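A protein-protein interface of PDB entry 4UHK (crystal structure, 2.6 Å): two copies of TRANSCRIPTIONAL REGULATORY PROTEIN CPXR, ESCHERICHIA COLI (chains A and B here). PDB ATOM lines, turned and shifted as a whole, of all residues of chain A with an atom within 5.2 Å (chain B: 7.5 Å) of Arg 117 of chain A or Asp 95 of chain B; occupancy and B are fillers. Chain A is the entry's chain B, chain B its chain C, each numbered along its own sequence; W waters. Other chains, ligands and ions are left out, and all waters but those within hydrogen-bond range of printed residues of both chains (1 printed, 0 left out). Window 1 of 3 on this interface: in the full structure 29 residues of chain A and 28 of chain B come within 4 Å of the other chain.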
ATOM      1  N   ASP A  96      21.097 -22.347 -23.207  1.00  0.00           N
ATOM      2  CA  ASP A  96      19.976 -22.367 -24.131  1.00  0.00           C
ATOM      3  C   ASP A  96      19.385 -23.784 -24.153  1.00  0.00           C
ATOM      4  O   ASP A  96      20.007 -24.742 -23.686  1.00  0.00           O
ATOM      5  CB  ASP A  96      20.389 -21.900 -25.549  1.00  0.00           C
ATOM      6  CG  ASP A  96      19.292 -21.222 -26.386  1.00  0.00           C
ATOM      7  OD1 ASP A  96      18.089 -21.496 -26.148  1.00  0.00           O
ATOM      8  OD2 ASP A  96      19.638 -20.447 -27.298  1.00  0.00           O
ATOM      9  N   ARG A 112      25.796 -19.208 -32.463  1.00  0.00           N
ATOM     10  CA  ARG A 112      26.477 -17.941 -32.693  1.00  0.00           C
ATOM     11  C   ARG A 112      26.155 -16.905 -31.631  1.00  0.00           C
ATOM     12  O   ARG A 112      27.052 -16.173 -31.235  1.00  0.00           O
ATOM     13  CB  ARG A 112      26.130 -17.425 -34.076  1.00  0.00           C
ATOM     14  CG  ARG A 112      26.884 -18.156 -35.171  1.00  0.00           C
ATOM     15  CD  ARG A 112      26.280 -17.979 -36.556  1.00  0.00           C
ATOM     16  NE  ARG A 112      26.110 -16.589 -36.993  1.00  0.00           N
ATOM     17  CZ  ARG A 112      27.019 -15.900 -37.670  1.00  0.00           C
ATOM     18  NH1 ARG A 112      28.207 -16.429 -37.930  1.00  0.00           N
ATOM     19  NH2 ARG A 112      26.760 -14.661 -38.064  1.00  0.00           N
ATOM     20  N   ALA A 113      24.922 -16.878 -31.119  1.00  0.00           N
ATOM     21  CA  ALA A 113      24.485 -15.950 -30.068  1.00  0.00           C
ATOM     22  C   ALA A 113      25.274 -16.163 -28.782  1.00  0.00           C
ATOM     23  O   ALA A 113      25.757 -15.192 -28.201  1.00  0.00           O
ATOM     24  CB  ALA A 113      23.001 -16.099 -29.808  1.00  0.00           C
ATOM     25  N   ILE A 114      25.475 -17.424 -28.375  1.00  0.00           N
ATOM     26  CA  ILE A 114      26.205 -17.712 -27.138  1.00  0.00           C
ATOM     27  C   ILE A 114      27.738 -17.605 -27.386  1.00  0.00           C
ATOM     28  O   ILE A 114      28.431 -17.109 -26.502  1.00  0.00           O
ATOM     29  CB  ILE A 114      25.757 -19.041 -26.425  1.00  0.00           C
ATOM     30  CG1 ILE A 114      26.392 -19.209 -25.018  1.00  0.00           C
ATOM     31  CG2 ILE A 114      25.951 -20.277 -27.248  1.00  0.00           C
ATOM     32  CD1 ILE A 114      26.133 -17.963 -23.871  1.00  0.00           C
ATOM     33  N   LEU A 115      28.245 -17.946 -28.586  1.00  0.00           N
ATOM     34  CA  LEU A 115      29.678 -17.821 -28.869  1.00  0.00           C
ATOM     35  C   LEU A 115      30.092 -16.349 -29.029  1.00  0.00           C
ATOM     36  O   LEU A 115      31.226 -16.005 -28.665  1.00  0.00           O
ATOM     37  CB  LEU A 115      30.119 -18.656 -30.064  1.00  0.00           C
ATOM     38  CG  LEU A 115      30.093 -20.179 -29.846  1.00  0.00           C
ATOM     39  CD1 LEU A 115      30.457 -20.918 -31.137  1.00  0.00           C
ATOM     40  CD2 LEU A 115      31.004 -20.626 -28.670  1.00  0.00           C
ATOM     41  N   ARG A 116      29.158 -15.472 -29.489  1.00  0.00           N
ATOM     42  CA  ARG A 116      29.376 -14.017 -29.585  1.00  0.00           C
ATOM     43  C   ARG A 116      29.536 -13.444 -28.166  1.00  0.00           C
ATOM     44  O   ARG A 116      30.396 -12.607 -27.938  1.00  0.00           O
ATOM     45  CB  ARG A 116      28.202 -13.353 -30.328  1.00  0.00           C
ATOM     46  CG  ARG A 116      28.225 -11.823 -30.404  1.00  0.00           C
ATOM     47  CD  ARG A 116      27.020 -11.269 -31.151  1.00  0.00           C
ATOM     48  NE  ARG A 116      25.772 -11.721 -30.542  1.00  0.00           N
ATOM     49  CZ  ARG A 116      24.652 -11.976 -31.205  1.00  0.00           C
ATOM     50  NH1 ARG A 116      24.595 -11.781 -32.515  1.00  0.00           N
ATOM     51  NH2 ARG A 116      23.578 -12.418 -30.565  1.00  0.00           N
ATOM     52  N   ARG A 117      28.715 -13.921 -27.224  1.00  0.00           N
ATOM     53  CA  ARG A 117      28.732 -13.521 -25.820  1.00  0.00           C
ATOM     54  C   ARG A 117      30.082 -13.936 -25.191  1.00  0.00           C
ATOM     55  O   ARG A 117      30.708 -13.127 -24.502  1.00  0.00           O
ATOM     56  CB  ARG A 117      27.517 -14.162 -25.111  1.00  0.00           C
ATOM     57  CG  ARG A 117      27.380 -13.973 -23.601  1.00  0.00           C
ATOM     58  CD  ARG A 117      27.259 -12.539 -23.114  1.00  0.00           C
ATOM     59  NE  ARG A 117      26.230 -11.777 -23.811  1.00  0.00           N
ATOM     60  CZ  ARG A 117      26.150 -10.456 -23.793  1.00  0.00           C
ATOM     61  NH1 ARG A 117      27.019  -9.741 -23.095  1.00  0.00           N
ATOM     62  NH2 ARG A 117      25.199  -9.836 -24.477  1.00  0.00           N
ATOM     63  N   SER A 118      30.545 -15.172 -25.493  1.00  0.00           N
ATOM     64  CA  SER A 118      31.823 -15.763 -25.052  1.00  0.00           C
ATOM     65  C   SER A 118      33.015 -14.913 -25.505  1.00  0.00           C
ATOM     66  O   SER A 118      33.889 -14.593 -24.695  1.00  0.00           O
ATOM     67  CB  SER A 118      31.976 -17.182 -25.601  1.00  0.00           C
ATOM     68  OG  SER A 118      31.300 -18.143 -24.811  1.00  0.00           O
ATOM     69  N   HIS A 119      33.016 -14.525 -26.798  1.00  0.00           N
ATOM     70  CA  HIS A 119      34.051 -13.707 -27.408  1.00  0.00           C
ATOM     71  C   HIS A 119      34.083 -12.304 -26.778  1.00  0.00           C
ATOM     72  O   HIS A 119      35.167 -11.801 -26.504  1.00  0.00           O
ATOM     73  CB  HIS A 119      33.847 -13.650 -28.927  1.00  0.00           C
ATOM     74  CG  HIS A 119      34.793 -12.740 -29.639  1.00  0.00           C
ATOM     75  ND1 HIS A 119      36.166 -13.007 -29.706  1.00  0.00           N
ATOM     76  CD2 HIS A 119      34.540 -11.581 -30.289  1.00  0.00           C
ATOM     77  CE1 HIS A 119      36.689 -11.997 -30.386  1.00  0.00           C
ATOM     78  NE2 HIS A 119      35.752 -11.121 -30.768  1.00  0.00           N
ATOM     79  N   TRP A 120      32.913 -11.693 -26.513  1.00  0.00           N
ATOM     80  CA  TRP A 120      32.823 -10.385 -25.876  1.00  0.00           C
ATOM     81  C   TRP A 120      33.456 -10.410 -24.491  1.00  0.00           C
ATOM     82  O   TRP A 120      34.156  -9.461 -24.125  1.00  0.00           O
ATOM     83  CB  TRP A 120      31.372  -9.924 -25.773  1.00  0.00           C
ATOM     84  CG  TRP A 120      30.779  -9.372 -27.044  1.00  0.00           C
ATOM     85  CD1 TRP A 120      31.445  -8.811 -28.098  1.00  0.00           C
ATOM     86  CD2 TRP A 120      29.387  -9.235 -27.335  1.00  0.00           C
ATOM     87  NE1 TRP A 120      30.552  -8.366 -29.040  1.00  0.00           N
ATOM     88  CE2 TRP A 120      29.280  -8.607 -28.598  1.00  0.00           C
ATOM     89  CE3 TRP A 120      28.216  -9.606 -26.663  1.00  0.00           C
ATOM     90  CZ2 TRP A 120      28.050  -8.357 -29.207  1.00  0.00           C
ATOM     91  CZ3 TRP A 120      26.996  -9.342 -27.258  1.00  0.00           C
ATOM     92  CH2 TRP A 120      26.919  -8.733 -28.520  1.00  0.00           C
ATOM     93  N   SER A 121      33.226 -11.519 -23.744  1.00  0.00           N
ATOM     94  CA  SER A 121      33.751 -11.807 -22.402  1.00  0.00           C
ATOM     95  C   SER A 121      35.273 -11.938 -22.426  1.00  0.00           C
ATOM     96  O   SER A 121      35.941 -11.431 -21.521  1.00  0.00           O
ATOM     97  CB  SER A 121      33.128 -13.088 -21.860  1.00  0.00           C
ATOM     98  OG  SER A 121      31.778 -12.880 -21.471  1.00  0.00           O
ATOM     99  N   ASP B  46      21.540  -4.691 -16.470  1.00  0.00           N
ATOM    100  CA  ASP B  46      22.136  -6.023 -16.569  1.00  0.00           C
ATOM    101  C   ASP B  46      21.524  -6.868 -17.687  1.00  0.00           C
ATOM    102  O   ASP B  46      22.182  -7.789 -18.174  1.00  0.00           O
ATOM    103  CB  ASP B  46      22.016  -6.765 -15.227  1.00  0.00           C
ATOM    104  CG  ASP B  46      22.746  -6.058 -14.105  1.00  0.00           C
ATOM    105  OD1 ASP B  46      23.972  -5.885 -14.212  1.00  0.00           O
ATOM    106  OD2 ASP B  46      22.085  -5.640 -13.143  1.00  0.00           O
ATOM    107  N   LEU B  47      20.268  -6.565 -18.074  1.00  0.00           N
ATOM    108  CA  LEU B  47      19.506  -7.275 -19.098  1.00  0.00           C
ATOM    109  C   LEU B  47      18.342  -6.422 -19.614  1.00  0.00           C
ATOM    110  O   LEU B  47      17.737  -5.672 -18.843  1.00  0.00           O
ATOM    111  CB  LEU B  47      18.962  -8.608 -18.509  1.00  0.00           C
ATOM    112  CG  LEU B  47      18.020  -9.443 -19.384  1.00  0.00           C
ATOM    113  CD1 LEU B  47      18.773 -10.498 -20.121  1.00  0.00           C
ATOM    114  CD2 LEU B  47      16.942 -10.072 -18.565  1.00  0.00           C
ATOM    115  N   LEU B  48      18.008  -6.597 -20.913  1.00  0.00           N
ATOM    116  CA  LEU B  48      16.874  -5.983 -21.609  1.00  0.00           C
ATOM    117  C   LEU B  48      15.884  -7.039 -22.062  1.00  0.00           C
ATOM    118  O   LEU B  48      16.273  -7.984 -22.744  1.00  0.00           O
ATOM    119  CB  LEU B  48      17.304  -5.165 -22.849  1.00  0.00           C
ATOM    120  CG  LEU B  48      18.127  -3.935 -22.619  1.00  0.00           C
ATOM    121  CD1 LEU B  48      18.536  -3.380 -23.868  1.00  0.00           C
ATOM    122  CD2 LEU B  48      17.339  -2.899 -22.128  1.00  0.00           C
ATOM    123  N   LEU B  63      17.579  -2.628 -31.026  1.00  0.00           N
ATOM    124  CA  LEU B  63      18.628  -3.630 -30.873  1.00  0.00           C
ATOM    125  C   LEU B  63      19.836  -3.253 -31.719  1.00  0.00           C
ATOM    126  O   LEU B  63      20.956  -3.248 -31.202  1.00  0.00           O
ATOM    127  CB  LEU B  63      18.085  -5.036 -31.256  1.00  0.00           C
ATOM    128  CG  LEU B  63      19.035  -6.255 -31.175  1.00  0.00           C
ATOM    129  CD1 LEU B  63      19.583  -6.460 -29.767  1.00  0.00           C
ATOM    130  CD2 LEU B  63      18.329  -7.497 -31.624  1.00  0.00           C
ATOM    131  N   ARG B  67      23.324  -2.117 -29.828  1.00  0.00           N
ATOM    132  CA  ARG B  67      24.466  -2.991 -30.116  1.00  0.00           C
ATOM    133  C   ARG B  67      25.668  -2.250 -30.726  1.00  0.00           C
ATOM    134  O   ARG B  67      26.758  -2.830 -30.794  1.00  0.00           O
ATOM    135  CB  ARG B  67      24.063  -4.168 -31.016  1.00  0.00           C
ATOM    136  CG  ARG B  67      23.458  -5.345 -30.255  1.00  0.00           C
ATOM    137  CD  ARG B  67      24.483  -6.072 -29.391  1.00  0.00           C
ATOM    138  NE  ARG B  67      23.863  -7.137 -28.612  1.00  0.00           N
ATOM    139  CZ  ARG B  67      23.569  -7.055 -27.322  1.00  0.00           C
ATOM    140  NH1 ARG B  67      23.899  -5.968 -26.630  1.00  0.00           N
ATOM    141  NH2 ARG B  67      22.969  -8.055 -26.708  1.00  0.00           N
ATOM    142  N   HIS B  70      26.582  -0.841 -26.788  1.00  0.00           N
ATOM    143  CA  HIS B  70      26.373  -1.699 -25.611  1.00  0.00           C
ATOM    144  C   HIS B  70      26.323  -3.188 -25.919  1.00  0.00           C
ATOM    145  O   HIS B  70      25.658  -3.624 -26.861  1.00  0.00           O
ATOM    146  CB  HIS B  70      25.079  -1.297 -24.899  1.00  0.00           C
ATOM    147  CG  HIS B  70      25.200   0.021 -24.198  1.00  0.00           C
ATOM    148  ND1 HIS B  70      25.144   1.223 -24.892  1.00  0.00           N
ATOM    149  CD2 HIS B  70      25.413   0.281 -22.890  1.00  0.00           C
ATOM    150  CE1 HIS B  70      25.296   2.167 -23.980  1.00  0.00           C
ATOM    151  NE2 HIS B  70      25.461   1.651 -22.761  1.00  0.00           N
ATOM    152  N   GLN B  71      27.013  -3.970 -25.079  1.00  0.00           N
ATOM    153  CA  GLN B  71      27.050  -5.432 -25.160  1.00  0.00           C
ATOM    154  C   GLN B  71      26.081  -6.034 -24.131  1.00  0.00           C
ATOM    155  O   GLN B  71      26.117  -7.236 -23.896  1.00  0.00           O
ATOM    156  CB  GLN B  71      28.476  -5.960 -24.919  1.00  0.00           C
ATOM    157  CG  GLN B  71      29.512  -5.622 -25.988  1.00  0.00           C
ATOM    158  CD  GLN B  71      30.907  -6.016 -25.531  1.00  0.00           C
ATOM    159  OE1 GLN B  71      31.147  -6.366 -24.355  1.00  0.00           O
ATOM    160  NE2 GLN B  71      31.868  -5.943 -26.448  1.00  0.00           N
ATOM    161  N   THR B  72      25.222  -5.185 -23.516  1.00  0.00           N
ATOM    162  CA  THR B  72      24.206  -5.559 -22.521  1.00  0.00           C
ATOM    163  C   THR B  72      23.395  -6.751 -23.000  1.00  0.00           C
ATOM    164  O   THR B  72      22.905  -6.713 -24.128  1.00  0.00           O
ATOM    165  CB  THR B  72      23.257  -4.376 -22.242  1.00  0.00           C
ATOM    166  OG1 THR B  72      24.014  -3.187 -22.072  1.00  0.00           O
ATOM    167  CG2 THR B  72      22.338  -4.606 -21.034  1.00  0.00           C
ATOM    168  N   PRO B  73      23.236  -7.817 -22.177  1.00  0.00           N
ATOM    169  CA  PRO B  73      22.413  -8.963 -22.611  1.00  0.00           C
ATOM    170  C   PRO B  73      20.971  -8.560 -22.961  1.00  0.00           C
ATOM    171  O   PRO B  73      20.378  -7.714 -22.286  1.00  0.00           O
ATOM    172  CB  PRO B  73      22.453  -9.903 -21.395  1.00  0.00           C
ATOM    173  CG  PRO B  73      23.705  -9.542 -20.688  1.00  0.00           C
ATOM    174  CD  PRO B  73      23.794  -8.054 -20.831  1.00  0.00           C
ATOM    175  N   VAL B  74      20.451  -9.078 -24.081  1.00  0.00           N
ATOM    176  CA  VAL B  74      19.071  -8.780 -24.467  1.00  0.00           C
ATOM    177  C   VAL B  74      18.374 -10.099 -24.849  1.00  0.00           C
ATOM    178  O   VAL B  74      18.996 -10.994 -25.423  1.00  0.00           O
ATOM    179  CB  VAL B  74      18.812  -7.610 -25.513  1.00  0.00           C
ATOM    180  CG1 VAL B  74      20.057  -6.791 -25.847  1.00  0.00           C
ATOM    181  CG2 VAL B  74      18.077  -8.069 -26.775  1.00  0.00           C
ATOM    182  N   ILE B  75      17.100 -10.214 -24.430  1.00  0.00           N
ATOM    183  CA  ILE B  75      16.165 -11.304 -24.716  1.00  0.00           C
ATOM    184  C   ILE B  75      14.985 -10.678 -25.446  1.00  0.00           C
ATOM    185  O   ILE B  75      14.301  -9.811 -24.876  1.00  0.00           O
ATOM    186  CB  ILE B  75      15.695 -12.099 -23.443  1.00  0.00           C
ATOM    187  CG1 ILE B  75      16.887 -12.689 -22.658  1.00  0.00           C
ATOM    188  CG2 ILE B  75      14.637 -13.186 -23.807  1.00  0.00           C
ATOM    189  CD1 ILE B  75      16.530 -13.377 -21.331  1.00  0.00           C
ATOM    190  N   MET B  76      14.725 -11.113 -26.676  1.00  0.00           N
ATOM    191  CA  MET B  76      13.559 -10.626 -27.392  1.00  0.00           C
ATOM    192  C   MET B  76      12.320 -11.336 -26.826  1.00  0.00           C
ATOM    193  O   MET B  76      12.333 -12.562 -26.681  1.00  0.00           O
ATOM    194  CB  MET B  76      13.687 -10.855 -28.906  1.00  0.00           C
ATOM    195  CG  MET B  76      14.963 -10.300 -29.533  1.00  0.00           C
ATOM    196  SD  MET B  76      15.141  -8.512 -29.435  1.00  0.00           S
ATOM    197  CE  MET B  76      13.890  -7.963 -30.613  1.00  0.00           C
ATOM    198  N   GLY B  89      16.450 -11.750 -34.879  1.00  0.00           N
ATOM    199  CA  GLY B  89      16.695 -11.195 -33.551  1.00  0.00           C
ATOM    200  C   GLY B  89      18.050 -11.602 -33.005  1.00  0.00           C
ATOM    201  O   GLY B  89      18.814 -10.756 -32.535  1.00  0.00           O
ATOM    202  N   LEU B  90      18.382 -12.892 -33.137  1.00  0.00           N
ATOM    203  CA  LEU B  90      19.616 -13.501 -32.668  1.00  0.00           C
ATOM    204  C   LEU B  90      20.799 -12.993 -33.441  1.00  0.00           C
ATOM    205  O   LEU B  90      21.799 -12.630 -32.832  1.00  0.00           O
ATOM    206  CB  LEU B  90      19.522 -15.033 -32.730  1.00  0.00           C
ATOM    207  CG  LEU B  90      18.547 -15.677 -31.701  1.00  0.00           C
ATOM    208  CD1 LEU B  90      18.066 -17.018 -32.193  1.00  0.00           C
ATOM    209  CD2 LEU B  90      19.167 -15.781 -30.340  1.00  0.00           C
ATOM    210  N   GLY B  93      21.837  -9.296 -32.644  1.00  0.00           N
ATOM    211  CA  GLY B  93      22.499  -9.040 -31.366  1.00  0.00           C
ATOM    212  C   GLY B  93      21.874  -9.615 -30.110  1.00  0.00           C
ATOM    213  O   GLY B  93      22.465  -9.496 -29.037  1.00  0.00           O
ATOM    214  N   ALA B  94      20.683 -10.244 -30.205  1.00  0.00           N
ATOM    215  CA  ALA B  94      20.006 -10.803 -29.023  1.00  0.00           C
ATOM    216  C   ALA B  94      20.645 -12.119 -28.574  1.00  0.00           C
ATOM    217  O   ALA B  94      21.081 -12.930 -29.397  1.00  0.00           O
ATOM    218  CB  ALA B  94      18.530 -11.000 -29.289  1.00  0.00           C
ATOM    219  N   ASP B  95      20.691 -12.308 -27.239  1.00  0.00           N
ATOM    220  CA  ASP B  95      21.275 -13.446 -26.540  1.00  0.00           C
ATOM    221  C   ASP B  95      20.298 -14.597 -26.436  1.00  0.00           C
ATOM    222  O   ASP B  95      20.715 -15.741 -26.242  1.00  0.00           O
ATOM    223  CB  ASP B  95      21.729 -13.018 -25.143  1.00  0.00           C
ATOM    224  CG  ASP B  95      22.850 -12.008 -25.208  1.00  0.00           C
ATOM    225  OD1 ASP B  95      24.024 -12.429 -25.377  1.00  0.00           O
ATOM    226  OD2 ASP B  95      22.551 -10.795 -25.202  1.00  0.00           O
ATOM    227  N   ASP B  96      18.995 -14.282 -26.501  1.00  0.00           N
ATOM    228  CA  ASP B  96      17.876 -15.216 -26.465  1.00  0.00           C
ATOM    229  C   ASP B  96      16.686 -14.559 -27.156  1.00  0.00           C
ATOM    230  O   ASP B  96      16.668 -13.343 -27.393  1.00  0.00           O
ATOM    231  CB  ASP B  96      17.521 -15.655 -25.018  1.00  0.00           C
ATOM    232  CG  ASP B  96      16.917 -17.052 -24.866  1.00  0.00           C
ATOM    233  OD1 ASP B  96      16.326 -17.563 -25.844  1.00  0.00           O
ATOM    234  OD2 ASP B  96      16.996 -17.611 -23.765  1.00  0.00           O
ATOM    235  N   TYR B  97      15.696 -15.384 -27.488  1.00  0.00           N
ATOM    236  CA  TYR B  97      14.490 -14.991 -28.193  1.00  0.00           C
ATOM    237  C   TYR B  97      13.370 -15.888 -27.729  1.00  0.00           C
ATOM    238  O   TYR B  97      13.427 -17.108 -27.931  1.00  0.00           O
ATOM    239  CB  TYR B  97      14.724 -15.119 -29.717  1.00  0.00           C
ATOM    240  CG  TYR B  97      13.780 -14.295 -30.562  1.00  0.00           C
ATOM    241  CD1 TYR B  97      12.438 -14.643 -30.686  1.00  0.00           C
ATOM    242  CD2 TYR B  97      14.246 -13.227 -31.314  1.00  0.00           C
ATOM    243  CE1 TYR B  97      11.571 -13.909 -31.489  1.00  0.00           C
ATOM    244  CE2 TYR B  97      13.385 -12.468 -32.100  1.00  0.00           C
ATOM    245  CZ  TYR B  97      12.048 -12.820 -32.196  1.00  0.00           C
ATOM    246  OH  TYR B  97      11.214 -12.086 -32.996  1.00  0.00           O
ATOM    247  N   ARG B 110      15.289 -18.418 -18.408  1.00  0.00           N
ATOM    248  CA  ARG B 110      16.102 -17.849 -19.487  1.00  0.00           C
ATOM    249  C   ARG B 110      16.815 -16.556 -19.022  1.00  0.00           C
ATOM    250  O   ARG B 110      17.980 -16.345 -19.371  1.00  0.00           O
ATOM    251  CB  ARG B 110      15.255 -17.599 -20.750  1.00  0.00           C
ATOM    252  CG  ARG B 110      14.795 -18.909 -21.364  1.00  0.00           C
ATOM    253  CD  ARG B 110      14.104 -18.827 -22.711  1.00  0.00           C
ATOM    254  NE  ARG B 110      13.879 -20.190 -23.217  1.00  0.00           N
ATOM    255  CZ  ARG B 110      14.741 -20.892 -23.953  1.00  0.00           C
ATOM    256  NH1 ARG B 110      15.896 -20.353 -24.336  1.00  0.00           N
ATOM    257  NH2 ARG B 110      14.450 -22.131 -24.323  1.00  0.00           N
ATOM    258  N   ILE B 114      21.131 -16.418 -18.675  1.00  0.00           N
ATOM    259  CA  ILE B 114      22.054 -15.436 -19.241  1.00  0.00           C
ATOM    260  C   ILE B 114      22.719 -14.609 -18.107  1.00  0.00           C
ATOM    261  O   ILE B 114      23.911 -14.316 -18.226  1.00  0.00           O
ATOM    262  CB  ILE B 114      21.439 -14.559 -20.395  1.00  0.00           C
ATOM    263  CG1 ILE B 114      22.505 -13.669 -21.109  1.00  0.00           C
ATOM    264  CG2 ILE B 114      20.246 -13.748 -19.979  1.00  0.00           C
ATOM    265  CD1 ILE B 114      23.809 -14.450 -21.815  1.00  0.00           C
ATOM    266  N   ARG B 117      25.616 -16.637 -16.696  1.00  0.00           N
ATOM    267  CA  ARG B 117      26.732 -16.557 -17.638  1.00  0.00           C
ATOM    268  C   ARG B 117      27.503 -15.235 -17.392  1.00  0.00           C
ATOM    269  O   ARG B 117      28.738 -15.251 -17.324  1.00  0.00           O
ATOM    270  CB  ARG B 117      26.180 -16.663 -19.074  1.00  0.00           C
ATOM    271  CG  ARG B 117      27.157 -16.460 -20.243  1.00  0.00           C
ATOM    272  CD  ARG B 117      28.306 -17.451 -20.339  1.00  0.00           C
ATOM    273  NE  ARG B 117      27.871 -18.846 -20.282  1.00  0.00           N
ATOM    274  CZ  ARG B 117      28.679 -19.864 -20.000  1.00  0.00           C
ATOM    275  NH1 ARG B 117      29.979 -19.654 -19.798  1.00  0.00           N
ATOM    276  NH2 ARG B 117      28.198 -21.097 -19.921  1.00  0.00           N
ATOM    277  N   SER B 118      26.757 -14.115 -17.199  1.00  0.00           N
ATOM    278  CA  SER B 118      27.276 -12.771 -16.920  1.00  0.00           C
ATOM    279  C   SER B 118      28.112 -12.754 -15.628  1.00  0.00           C
ATOM    280  O   SER B 118      29.225 -12.223 -15.609  1.00  0.00           O
ATOM    281  CB  SER B 118      26.123 -11.775 -16.807  1.00  0.00           C
ATOM    282  OG  SER B 118      25.681 -11.307 -18.072  1.00  0.00           O
ATOM    283  N   SER B 121      31.431 -14.655 -15.949  1.00  0.00           N
ATOM    284  CA  SER B 121      32.298 -13.776 -16.738  1.00  0.00           C
ATOM    285  C   SER B 121      32.951 -12.712 -15.841  1.00  0.00           C
ATOM    286  O   SER B 121      34.144 -12.431 -15.991  1.00  0.00           O
ATOM    287  CB  SER B 121      31.476 -13.132 -17.854  1.00  0.00           C
ATOM    288  OG  SER B 121      32.125 -12.086 -18.549  1.00  0.00           O
HETATM  289  O   HOH W   1      24.996 -12.562 -28.065  1.00  0.00           O
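Printed residues of chain B within 4 Å of Asp 96 of chain A: Arg 110.
Arg 117 of chain A touches just these residues of chain B: Arg 67, Gln 71, Thr 72, Pro 73 and Asp 95.
His 119 of chain A touches none of the printed residues of chain B.
Of the printed residues of chain B, Trp 120 of chain A touches Arg 67 (3.4 Å) and Gln 71 (3.3 Å).
Asp 95 of chain B touches one residue of chain A.
The nearest printed residue of chain A that does not touch Ser 121 of chain B is Arg 117 of chain A (6.2 Å).
Among the printed residues, merely in contact across the chains: Trp 120 of chain A with Gln 71 of chain B (3.3 Å), Trp 120 of chain A with Arg 67 of chain B (3.4 Å), Arg 117 of chain A with Pro 73 of chain B (3.5 Å), Arg 117 of chain A with Arg 67 of chain B (3.6 Å), Ala 113 of chain A with Ala 94 of chain B (3.7 Å), Arg 117 of chain A with Thr 72 of chain B (3.9 Å) and Ala 113 of chain A with Leu 90 of chain B (3.9 Å).
Ser 121 of chain A touches its own counterpart, Ser 121 of chain B.
5 positions are printed for both chains.
The backbone NH of Leu 48 of chain B is in hydrogen-bond range of the backbone carbonyl oxygen of Pro 73 of chain B (3.0 Å).
NH1 of Arg 67 of chain B lies within hydrogen-bond range of O of His 70 of chain B, 2.9 Å away.
NE of Arg 67 of chain B sits at hydrogen-bond distance from O of Gly 93 of chain B, 2.8 Å away.
The backbone NH (N) of Asp 95 of chain B sits at hydrogen-bond distance from the backbone carbonyl oxygen (O) of Val 74 of chain B, at 2.8 Å.
OD2 of Asp 96 of chain B is in salt-bridge range of NH1 of Arg 110 of chain B (3.0 Å).
The backbone carbonyl oxygen (O) of Gly 89 of chain B sits at hydrogen-bond distance from the backbone NH (N) of Ala 94 of chain B, 3.0 Å away.
NH2 of Arg 116 of chain A sits close to O of Gly 93 of chain B.
The side-chain hydroxyl (OG) of Ser 121 of chain A lies within hydrogen-bond range of the side-chain hydroxyl (OG) of Ser 121 of chain B (3.0 Å).
The side-chain carboxylate (OD1) of Asp 96 of chain A is in salt-bridge range of the guanidinium group (NH1) of Arg 110 of chain B, 3.1 Å away.
O of Leu 90 of chain B sits at hydrogen-bond distance from NH2 of Arg 116 of chain A, at 2.9 Å.
NH1 of Arg 117 of chain A is in hydrogen-bond range of O of Gln 71 of chain B, 2.8 Å away.
NH2 of Arg 116 of chain A sits at hydrogen-bond distance from O of Ala 94 of chain B (2.8 Å).
The guanidinium group (NE) of Arg 117 of chain A is in salt-bridge range of the side-chain carboxylate (OD1) of Asp 95 of chain B (2.8 Å).
Water W1 lies within hydrogen-bond range of NE of Arg 116 of chain A (2.7 Å), O of Ala 113 of chain A (2.7 Å) and OD1 of Asp 95 of chain B (2.9 Å).
Printed residues of chain A that touch a printed residue of chain B: Asp 96, Ala 113, Arg 116, Arg 117, Trp 120 and Ser 121.
Of the 24 printed residues of chain B, 10 touch a printed residue of chain A.
Printed residues of chain B that touch a printed residue of chain A: Arg 67, Gln 71, Thr 72, Pro 73, Leu 90, Gly 93, Ala 94, Asp 95, Arg 110 and Ser 121.
Along chain B the printed residues that touch a printed residue of chain A span positions 67 to 121.
Among the printed residues, Asp or Glu carboxylates within 4 Å of a Lys or Arg side-chain nitrogen of the other chain: Asp 96 of chain A with Arg 110 of chain B and Arg 117 of chain A with Asp 95 of chain B.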
